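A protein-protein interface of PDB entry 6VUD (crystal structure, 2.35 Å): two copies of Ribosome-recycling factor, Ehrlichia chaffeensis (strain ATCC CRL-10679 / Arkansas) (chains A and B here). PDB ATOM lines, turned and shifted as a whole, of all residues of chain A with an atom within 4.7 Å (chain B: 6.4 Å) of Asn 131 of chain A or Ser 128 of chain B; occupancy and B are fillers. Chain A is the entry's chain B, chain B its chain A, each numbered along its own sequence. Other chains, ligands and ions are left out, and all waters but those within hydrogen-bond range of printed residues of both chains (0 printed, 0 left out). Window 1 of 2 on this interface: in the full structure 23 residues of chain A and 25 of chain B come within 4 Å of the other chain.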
ATOM      1  N   VAL A 127     -10.867 -17.346  25.058  1.00  0.00           N
ATOM      2  CA  VAL A 127     -11.908 -17.698  24.097  1.00  0.00           C
ATOM      3  C   VAL A 127     -13.273 -17.260  24.617  1.00  0.00           C
ATOM      4  O   VAL A 127     -14.077 -16.675  23.881  1.00  0.00           O
ATOM      5  CB  VAL A 127     -11.867 -19.208  23.801  1.00  0.00           C
ATOM      6  CG1 VAL A 127     -13.180 -19.672  23.189  1.00  0.00           C
ATOM      7  CG2 VAL A 127     -10.715 -19.526  22.863  1.00  0.00           C
ATOM      8  N   SER A 128     -13.530 -17.493  25.907  1.00  0.00           N
ATOM      9  CA  SER A 128     -14.794 -17.089  26.514  1.00  0.00           C
ATOM     10  C   SER A 128     -14.988 -15.574  26.433  1.00  0.00           C
ATOM     11  O   SER A 128     -16.058 -15.091  26.033  1.00  0.00           O
ATOM     12  CB  SER A 128     -14.842 -17.587  27.963  1.00  0.00           C
ATOM     13  OG  SER A 128     -15.912 -17.011  28.690  1.00  0.00           O
ATOM     14  N   ILE A 129     -13.951 -14.809  26.792  1.00  0.00           N
ATOM     15  CA  ILE A 129     -14.034 -13.348  26.783  1.00  0.00           C
ATOM     16  C   ILE A 129     -14.294 -12.834  25.370  1.00  0.00           C
ATOM     17  O   ILE A 129     -15.147 -11.966  25.153  1.00  0.00           O
ATOM     18  CB  ILE A 129     -12.745 -12.738  27.361  1.00  0.00           C
ATOM     19  CG1 ILE A 129     -12.497 -13.233  28.785  1.00  0.00           C
ATOM     20  CG2 ILE A 129     -12.777 -11.212  27.262  1.00  0.00           C
ATOM     21  CD1 ILE A 129     -13.439 -12.699  29.764  1.00  0.00           C
ATOM     22  N   ARG A 130     -13.544 -13.352  24.389  1.00  0.00           N
ATOM     23  CA  ARG A 130     -13.715 -12.917  23.006  1.00  0.00           C
ATOM     24  C   ARG A 130     -15.080 -13.325  22.456  1.00  0.00           C
ATOM     25  O   ARG A 130     -15.726 -12.545  21.747  1.00  0.00           O
ATOM     26  CB  ARG A 130     -12.577 -13.478  22.148  1.00  0.00           C
ATOM     27  CG  ARG A 130     -11.217 -12.856  22.511  1.00  0.00           C
ATOM     28  CD  ARG A 130     -10.142 -13.090  21.443  1.00  0.00           C
ATOM     29  NE  ARG A 130      -9.729 -14.484  21.362  1.00  0.00           N
ATOM     30  CZ  ARG A 130      -8.593 -14.973  21.865  1.00  0.00           C
ATOM     31  NH1 ARG A 130      -7.726 -14.180  22.491  1.00  0.00           N
ATOM     32  NH2 ARG A 130      -8.324 -16.266  21.740  1.00  0.00           N
ATOM     33  N   ASN A 131     -15.531 -14.539  22.773  1.00  0.00           N
ATOM     34  CA  ASN A 131     -16.873 -14.959  22.396  1.00  0.00           C
ATOM     35  C   ASN A 131     -17.931 -14.012  22.969  1.00  0.00           C
ATOM     36  O   ASN A 131     -18.853 -13.602  22.255  1.00  0.00           O
ATOM     37  CB  ASN A 131     -17.116 -16.396  22.857  1.00  0.00           C
ATOM     38  CG  ASN A 131     -18.344 -17.012  22.210  1.00  0.00           C
ATOM     39  OD1 ASN A 131     -18.508 -16.951  20.989  1.00  0.00           O
ATOM     40  ND2 ASN A 131     -19.226 -17.584  23.029  1.00  0.00           N
ATOM     41  N   ILE A 132     -17.795 -13.630  24.244  1.00  0.00           N
ATOM     42  CA  ILE A 132     -18.755 -12.708  24.850  1.00  0.00           C
ATOM     43  C   ILE A 132     -18.757 -11.383  24.105  1.00  0.00           C
ATOM     44  O   ILE A 132     -19.819 -10.820  23.811  1.00  0.00           O
ATOM     45  CB  ILE A 132     -18.454 -12.511  26.350  1.00  0.00           C
ATOM     46  CG1 ILE A 132     -18.729 -13.790  27.149  1.00  0.00           C
ATOM     47  CG2 ILE A 132     -19.263 -11.347  26.937  1.00  0.00           C
ATOM     48  CD1 ILE A 132     -18.242 -13.718  28.608  1.00  0.00           C
ATOM     49  N   ARG A 133     -17.574 -10.861  23.784  1.00  0.00           N
ATOM     50  CA  ARG A 133     -17.505  -9.612  23.040  1.00  0.00           C
ATOM     51  C   ARG A 133     -18.228  -9.734  21.698  1.00  0.00           C
ATOM     52  O   ARG A 133     -19.046  -8.874  21.345  1.00  0.00           O
ATOM     53  CB  ARG A 133     -16.048  -9.194  22.844  1.00  0.00           C
ATOM     54  CG  ARG A 133     -15.895  -7.818  22.226  1.00  0.00           C
ATOM     55  CD  ARG A 133     -14.454  -7.519  21.890  1.00  0.00           C
ATOM     56  NE  ARG A 133     -14.353  -6.899  20.578  1.00  0.00           N
ATOM     57  CZ  ARG A 133     -14.390  -7.579  19.438  1.00  0.00           C
ATOM     58  NH1 ARG A 133     -14.510  -8.902  19.459  1.00  0.00           N
ATOM     59  NH2 ARG A 133     -14.307  -6.942  18.276  1.00  0.00           N
ATOM     60  N   ARG A 134     -17.942 -10.805  20.943  1.00  0.00           N
ATOM     61  CA  ARG A 134     -18.648 -11.052  19.682  1.00  0.00           C
ATOM     62  C   ARG A 134     -20.157 -11.153  19.890  1.00  0.00           C
ATOM     63  O   ARG A 134     -20.936 -10.647  19.076  1.00  0.00           O
ATOM     64  CB  ARG A 134     -18.153 -12.341  19.013  1.00  0.00           C
ATOM     65  CG  ARG A 134     -16.896 -12.218  18.191  1.00  0.00           C
ATOM     66  CD  ARG A 134     -16.776 -13.377  17.185  1.00  0.00           C
ATOM     67  NE  ARG A 134     -17.019 -14.696  17.774  1.00  0.00           N
ATOM     68  CZ  ARG A 134     -16.115 -15.389  18.466  1.00  0.00           C
ATOM     69  NH1 ARG A 134     -14.904 -14.884  18.676  1.00  0.00           N
ATOM     70  NH2 ARG A 134     -16.425 -16.583  18.962  1.00  0.00           N
ATOM     71  N   ASP A 135     -20.586 -11.834  20.953  1.00  0.00           N
ATOM     72  CA  ASP A 135     -22.014 -12.000  21.207  1.00  0.00           C
ATOM     73  C   ASP A 135     -22.679 -10.664  21.514  1.00  0.00           C
ATOM     74  O   ASP A 135     -23.743 -10.343  20.969  1.00  0.00           O
ATOM     75  CB  ASP A 135     -22.220 -12.970  22.361  1.00  0.00           C
ATOM     76  CG  ASP A 135     -23.674 -13.099  22.752  1.00  0.00           C
ATOM     77  OD1 ASP A 135     -24.459 -13.540  21.895  1.00  0.00           O
ATOM     78  OD2 ASP A 135     -24.028 -12.761  23.907  1.00  0.00           O
ATOM     79  N   ARG B  13     -22.538 -24.054  34.811  1.00  0.00           N
ATOM     80  CA  ARG B  13     -22.064 -23.095  33.816  1.00  0.00           C
ATOM     81  C   ARG B  13     -22.801 -23.262  32.488  1.00  0.00           C
ATOM     82  O   ARG B  13     -23.095 -22.270  31.810  1.00  0.00           O
ATOM     83  CB  ARG B  13     -20.549 -23.230  33.628  1.00  0.00           C
ATOM     84  CG  ARG B  13     -19.717 -22.653  34.779  1.00  0.00           C
ATOM     85  CD  ARG B  13     -18.254 -23.148  34.761  1.00  0.00           C
ATOM     86  NE  ARG B  13     -17.558 -22.773  33.529  1.00  0.00           N
ATOM     87  CZ  ARG B  13     -16.293 -23.078  33.249  1.00  0.00           C
ATOM     88  NH1 ARG B  13     -15.759 -22.688  32.097  1.00  0.00           N
ATOM     89  NH2 ARG B  13     -15.560 -23.768  34.116  1.00  0.00           N
ATOM     90  N   MET B  14     -23.124 -24.503  32.107  1.00  0.00           N
ATOM     91  CA  MET B  14     -23.808 -24.724  30.835  1.00  0.00           C
ATOM     92  C   MET B  14     -25.245 -24.223  30.883  1.00  0.00           C
ATOM     93  O   MET B  14     -25.701 -23.538  29.960  1.00  0.00           O
ATOM     94  CB  MET B  14     -23.766 -26.203  30.457  1.00  0.00           C
ATOM     95  CG  MET B  14     -22.419 -26.639  29.918  1.00  0.00           C
ATOM     96  SD  MET B  14     -22.384 -28.380  29.444  1.00  0.00           S
ATOM     97  CE  MET B  14     -20.669 -28.571  29.003  1.00  0.00           C
ATOM     98  N   SER B  17     -25.311 -20.508  30.874  1.00  0.00           N
ATOM     99  CA  SER B  17     -24.979 -19.941  29.573  1.00  0.00           C
ATOM    100  C   SER B  17     -26.158 -20.046  28.616  1.00  0.00           C
ATOM    101  O   SER B  17     -26.537 -19.058  27.977  1.00  0.00           O
ATOM    102  CB  SER B  17     -23.746 -20.629  28.998  1.00  0.00           C
ATOM    103  OG  SER B  17     -23.425 -20.084  27.731  1.00  0.00           O
ATOM    104  N   LEU B  18     -26.755 -21.235  28.503  1.00  0.00           N
ATOM    105  CA  LEU B  18     -27.981 -21.371  27.720  1.00  0.00           C
ATOM    106  C   LEU B  18     -29.042 -20.387  28.195  1.00  0.00           C
ATOM    107  O   LEU B  18     -29.769 -19.795  27.384  1.00  0.00           O
ATOM    108  CB  LEU B  18     -28.510 -22.803  27.814  1.00  0.00           C
ATOM    109  CG  LEU B  18     -29.910 -23.020  27.229  1.00  0.00           C
ATOM    110  CD1 LEU B  18     -29.913 -22.756  25.729  1.00  0.00           C
ATOM    111  CD2 LEU B  18     -30.438 -24.415  27.535  1.00  0.00           C
ATOM    112  N   TYR B  21     -28.325 -16.970  26.750  1.00  0.00           N
ATOM    113  CA  TYR B  21     -28.593 -16.854  25.322  1.00  0.00           C
ATOM    114  C   TYR B  21     -30.088 -16.894  25.004  1.00  0.00           C
ATOM    115  O   TYR B  21     -30.526 -16.255  24.043  1.00  0.00           O
ATOM    116  CB  TYR B  21     -27.836 -17.950  24.570  1.00  0.00           C
ATOM    117  CG  TYR B  21     -26.370 -17.599  24.392  1.00  0.00           C
ATOM    118  CD1 TYR B  21     -25.422 -17.935  25.358  1.00  0.00           C
ATOM    119  CD2 TYR B  21     -25.942 -16.882  23.279  1.00  0.00           C
ATOM    120  CE1 TYR B  21     -24.070 -17.584  25.204  1.00  0.00           C
ATOM    121  CE2 TYR B  21     -24.604 -16.529  23.116  1.00  0.00           C
ATOM    122  CZ  TYR B  21     -23.677 -16.881  24.079  1.00  0.00           C
ATOM    123  OH  TYR B  21     -22.368 -16.508  23.903  1.00  0.00           O
ATOM    124  N   GLU B 123     -24.104 -19.661  17.204  1.00  0.00           N
ATOM    125  CA  GLU B 123     -22.763 -20.229  17.255  1.00  0.00           C
ATOM    126  C   GLU B 123     -21.985 -19.691  18.453  1.00  0.00           C
ATOM    127  O   GLU B 123     -21.198 -20.427  19.060  1.00  0.00           O
ATOM    128  CB  GLU B 123     -22.020 -19.956  15.942  1.00  0.00           C
ATOM    129  CG  GLU B 123     -20.656 -20.658  15.831  1.00  0.00           C
ATOM    130  CD  GLU B 123     -20.759 -22.182  15.736  1.00  0.00           C
ATOM    131  OE1 GLU B 123     -21.870 -22.714  15.514  1.00  0.00           O
ATOM    132  OE2 GLU B 123     -19.722 -22.858  15.888  1.00  0.00           O
ATOM    133  N   ASP B 124     -22.194 -18.416  18.815  1.00  0.00           N
ATOM    134  CA  ASP B 124     -21.626 -17.912  20.063  1.00  0.00           C
ATOM    135  C   ASP B 124     -22.079 -18.747  21.254  1.00  0.00           C
ATOM    136  O   ASP B 124     -21.312 -18.937  22.211  1.00  0.00           O
ATOM    137  CB  ASP B 124     -22.018 -16.455  20.301  1.00  0.00           C
ATOM    138  CG  ASP B 124     -21.559 -15.531  19.202  1.00  0.00           C
ATOM    139  OD1 ASP B 124     -20.504 -15.803  18.595  1.00  0.00           O
ATOM    140  OD2 ASP B 124     -22.257 -14.518  18.963  1.00  0.00           O
ATOM    141  N   CYS B 125     -23.322 -19.244  21.219  1.00  0.00           N
ATOM    142  CA  CYS B 125     -23.803 -20.113  22.288  1.00  0.00           C
ATOM    143  C   CYS B 125     -23.080 -21.456  22.272  1.00  0.00           C
ATOM    144  O   CYS B 125     -22.563 -21.902  23.303  1.00  0.00           O
ATOM    145  CB  CYS B 125     -25.317 -20.306  22.170  1.00  0.00           C
ATOM    146  SG  CYS B 125     -26.044 -21.171  23.571  1.00  0.00           S
ATOM    147  N   ARG B 126     -23.023 -22.114  21.110  1.00  0.00           N
ATOM    148  CA  ARG B 126     -22.307 -23.385  21.022  1.00  0.00           C
ATOM    149  C   ARG B 126     -20.864 -23.241  21.484  1.00  0.00           C
ATOM    150  O   ARG B 126     -20.336 -24.128  22.164  1.00  0.00           O
ATOM    151  CB  ARG B 126     -22.346 -23.928  19.596  1.00  0.00           C
ATOM    152  CG  ARG B 126     -23.742 -24.117  19.079  1.00  0.00           C
ATOM    153  CD  ARG B 126     -23.760 -24.909  17.793  1.00  0.00           C
ATOM    154  NE  ARG B 126     -25.122 -24.974  17.296  1.00  0.00           N
ATOM    155  CZ  ARG B 126     -25.680 -24.039  16.536  1.00  0.00           C
ATOM    156  NH1 ARG B 126     -24.980 -22.976  16.160  1.00  0.00           N
ATOM    157  NH2 ARG B 126     -26.942 -24.166  16.147  1.00  0.00           N
ATOM    158  N   VAL B 127     -20.216 -22.125  21.139  1.00  0.00           N
ATOM    159  CA  VAL B 127     -18.818 -21.941  21.516  1.00  0.00           C
ATOM    160  C   VAL B 127     -18.670 -21.925  23.032  1.00  0.00           C
ATOM    161  O   VAL B 127     -17.774 -22.573  23.584  1.00  0.00           O
ATOM    162  CB  VAL B 127     -18.244 -20.667  20.870  1.00  0.00           C
ATOM    163  CG1 VAL B 127     -16.906 -20.299  21.503  1.00  0.00           C
ATOM    164  CG2 VAL B 127     -18.067 -20.871  19.378  1.00  0.00           C
ATOM    165  N   SER B 128     -19.561 -21.219  23.736  1.00  0.00           N
ATOM    166  CA  SER B 128     -19.443 -21.179  25.189  1.00  0.00           C
ATOM    167  C   SER B 128     -19.714 -22.545  25.807  1.00  0.00           C
ATOM    168  O   SER B 128     -19.076 -22.905  26.802  1.00  0.00           O
ATOM    169  CB  SER B 128     -20.377 -20.118  25.781  1.00  0.00           C
ATOM    170  OG  SER B 128     -21.719 -20.546  25.805  1.00  0.00           O
ATOM    171  N   ILE B 129     -20.627 -23.324  25.222  1.00  0.00           N
ATOM    172  CA  ILE B 129     -20.929 -24.651  25.756  1.00  0.00           C
ATOM    173  C   ILE B 129     -19.746 -25.589  25.546  1.00  0.00           C
ATOM    174  O   ILE B 129     -19.357 -26.334  26.454  1.00  0.00           O
ATOM    175  CB  ILE B 129     -22.228 -25.200  25.129  1.00  0.00           C
ATOM    176  CG1 ILE B 129     -23.414 -24.299  25.480  1.00  0.00           C
ATOM    177  CG2 ILE B 129     -22.521 -26.617  25.611  1.00  0.00           C
ATOM    178  CD1 ILE B 129     -23.545 -24.028  26.971  1.00  0.00           C
ATOM    179  N   ARG B 130     -19.142 -25.555  24.359  1.00  0.00           N
ATOM    180  CA  ARG B 130     -17.938 -26.345  24.130  1.00  0.00           C
ATOM    181  C   ARG B 130     -16.776 -25.852  24.990  1.00  0.00           C
ATOM    182  O   ARG B 130     -16.009 -26.659  25.527  1.00  0.00           O
ATOM    183  CB  ARG B 130     -17.567 -26.315  22.647  1.00  0.00           C
ATOM    184  CG  ARG B 130     -18.588 -26.979  21.736  1.00  0.00           C
ATOM    185  CD  ARG B 130     -18.050 -27.153  20.322  1.00  0.00           C
ATOM    186  NE  ARG B 130     -18.244 -25.966  19.495  1.00  0.00           N
ATOM    187  CZ  ARG B 130     -19.217 -25.824  18.600  1.00  0.00           C
ATOM    188  NH1 ARG B 130     -19.301 -24.707  17.896  1.00  0.00           N
ATOM    189  NH2 ARG B 130     -20.106 -26.796  18.405  1.00  0.00           N
ATOM    190  N   ASN B 131     -16.635 -24.530  25.136  1.00  0.00           N
ATOM    191  CA  ASN B 131     -15.529 -23.986  25.918  1.00  0.00           C
ATOM    192  C   ASN B 131     -15.662 -24.355  27.387  1.00  0.00           C
ATOM    193  O   ASN B 131     -14.665 -24.663  28.048  1.00  0.00           O
ATOM    194  CB  ASN B 131     -15.459 -22.468  25.759  1.00  0.00           C
ATOM    195  CG  ASN B 131     -14.134 -21.909  26.205  1.00  0.00           C
ATOM    196  OD1 ASN B 131     -13.082 -22.336  25.726  1.00  0.00           O
ATOM    197  ND2 ASN B 131     -14.168 -20.964  27.134  1.00  0.00           N
ATOM    198  N   ILE B 132     -16.887 -24.330  27.914  1.00  0.00           N
ATOM    199  CA  ILE B 132     -17.122 -24.828  29.266  1.00  0.00           C
ATOM    200  C   ILE B 132     -16.687 -26.285  29.371  1.00  0.00           C
ATOM    201  O   ILE B 132     -16.000 -26.681  30.320  1.00  0.00           O
ATOM    202  CB  ILE B 132     -18.601 -24.654  29.657  1.00  0.00           C
ATOM    203  CG1 ILE B 132     -18.934 -23.170  29.839  1.00  0.00           C
ATOM    204  CG2 ILE B 132     -18.918 -25.446  30.922  1.00  0.00           C
ATOM    205  CD1 ILE B 132     -20.416 -22.882  29.952  1.00  0.00           C
ATOM    206  N   ARG B 133     -17.064 -27.100  28.385  1.00  0.00           N
ATOM    207  CA  ARG B 133     -16.709 -28.513  28.420  1.00  0.00           C
ATOM    208  C   ARG B 133     -15.195 -28.703  28.398  1.00  0.00           C
ATOM    209  O   ARG B 133     -14.648 -29.475  29.191  1.00  0.00           O
ATOM    210  CB  ARG B 133     -17.362 -29.255  27.254  1.00  0.00           C
ATOM    211  CG  ARG B 133     -17.071 -30.748  27.258  1.00  0.00           C
ATOM    212  CD  ARG B 133     -17.350 -31.387  25.912  1.00  0.00           C
ATOM    213  NE  ARG B 133     -16.259 -32.275  25.517  1.00  0.00           N
ATOM    214  CZ  ARG B 133     -15.208 -31.889  24.798  1.00  0.00           C
ATOM    215  NH1 ARG B 133     -15.109 -30.631  24.386  1.00  0.00           N
ATOM    216  NH2 ARG B 133     -14.259 -32.759  24.487  1.00  0.00           N
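Of chain B, only Tyr 21, Asp 124, Val 127 and Ser 128 come within 4 Å of Asn 131 of chain A.
Ser 128 of chain B touches just one residue of chain A: Asn 131.
Of the printed residues of chain A, Asp 124 of chain B touches Asn 131, Arg 134 and Asp 135.
Of the printed residues of chain B, Asp 135 of chain A touches Tyr 21 (3.2 Å) and Asp 124 (3.4 Å).
The nearest printed residue of chain B that does not touch Asp 135 of chain A is Cys 125 of chain B (5.9 Å).
Val 127 of chain A touches Asn 131 of chain B, and with the chains exchanged Asn 131 of chain A touches Val 127 of chain B.
Ser 128 of chain A touches Asn 131 of chain B, and with the chains exchanged Asn 131 of chain A touches Ser 128 of chain B.
Of the 9 pairs that touch across the chains among the printed residues, 4 have their exchanged pair printed and touching as well.
Among the printed residues, merely in contact across the chains: Asp 135 of chain A with Tyr 21 of chain B, Asp 135 of chain A with Asp 124 of chain B, Ser 128 of chain A with Asn 131 of chain B, Asn 131 of chain A with Val 127 of chain B, Val 127 of chain A with Asn 131 of chain B and Asn 131 of chain A with Ser 128 of chain B.
Printed residues of chain B that touch a printed residue of chain A: Tyr 21, Asp 124, Val 127, Ser 128 and Asn 131.
Hydrophobic or aromatic side chains of chain B within 4 Å of the printed part of chain A: Tyr 21 and Val 127.
Among the printed residues, 9 pairs touch across the chains.
The side-chain hydroxyl of Tyr 21 of chain B is in hydrogen-bond range of the side-chain amide nitrogen of Asn 131 of chain A (3.4 Å).
The backbone carbonyl oxygen (O) of Asp 124 of chain B lies within hydrogen-bond range of the side-chain amide nitrogen (ND2) of Asn 131 of chain A, at 2.6 Å.
OD1 of Asp 124 of chain B lies within salt-bridge range of NE of Arg 134 of chain A (3.7 Å).
The side-chain hydroxyl (OG) of Ser 128 of chain B sits at hydrogen-bond distance from the side-chain hydroxyl (OG) of Ser 17 of chain B (2.6 Å).
The backbone carbonyl oxygen (O) of Asp 124 of chain B sits at hydrogen-bond distance from the side-chain hydroxyl (OH) of Tyr 21 of chain B, 3.1 Å away.
The side-chain hydroxyl of Ser 128 of chain B is in hydrogen-bond range of the backbone carbonyl oxygen of Cys 125 of chain B (3.0 Å).
The side-chain amide oxygen (OD1) of Asn 131 of chain A sits at hydrogen-bond distance from the guanidinium group (NH2) of Arg 134 of chain A (2.9 Å).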
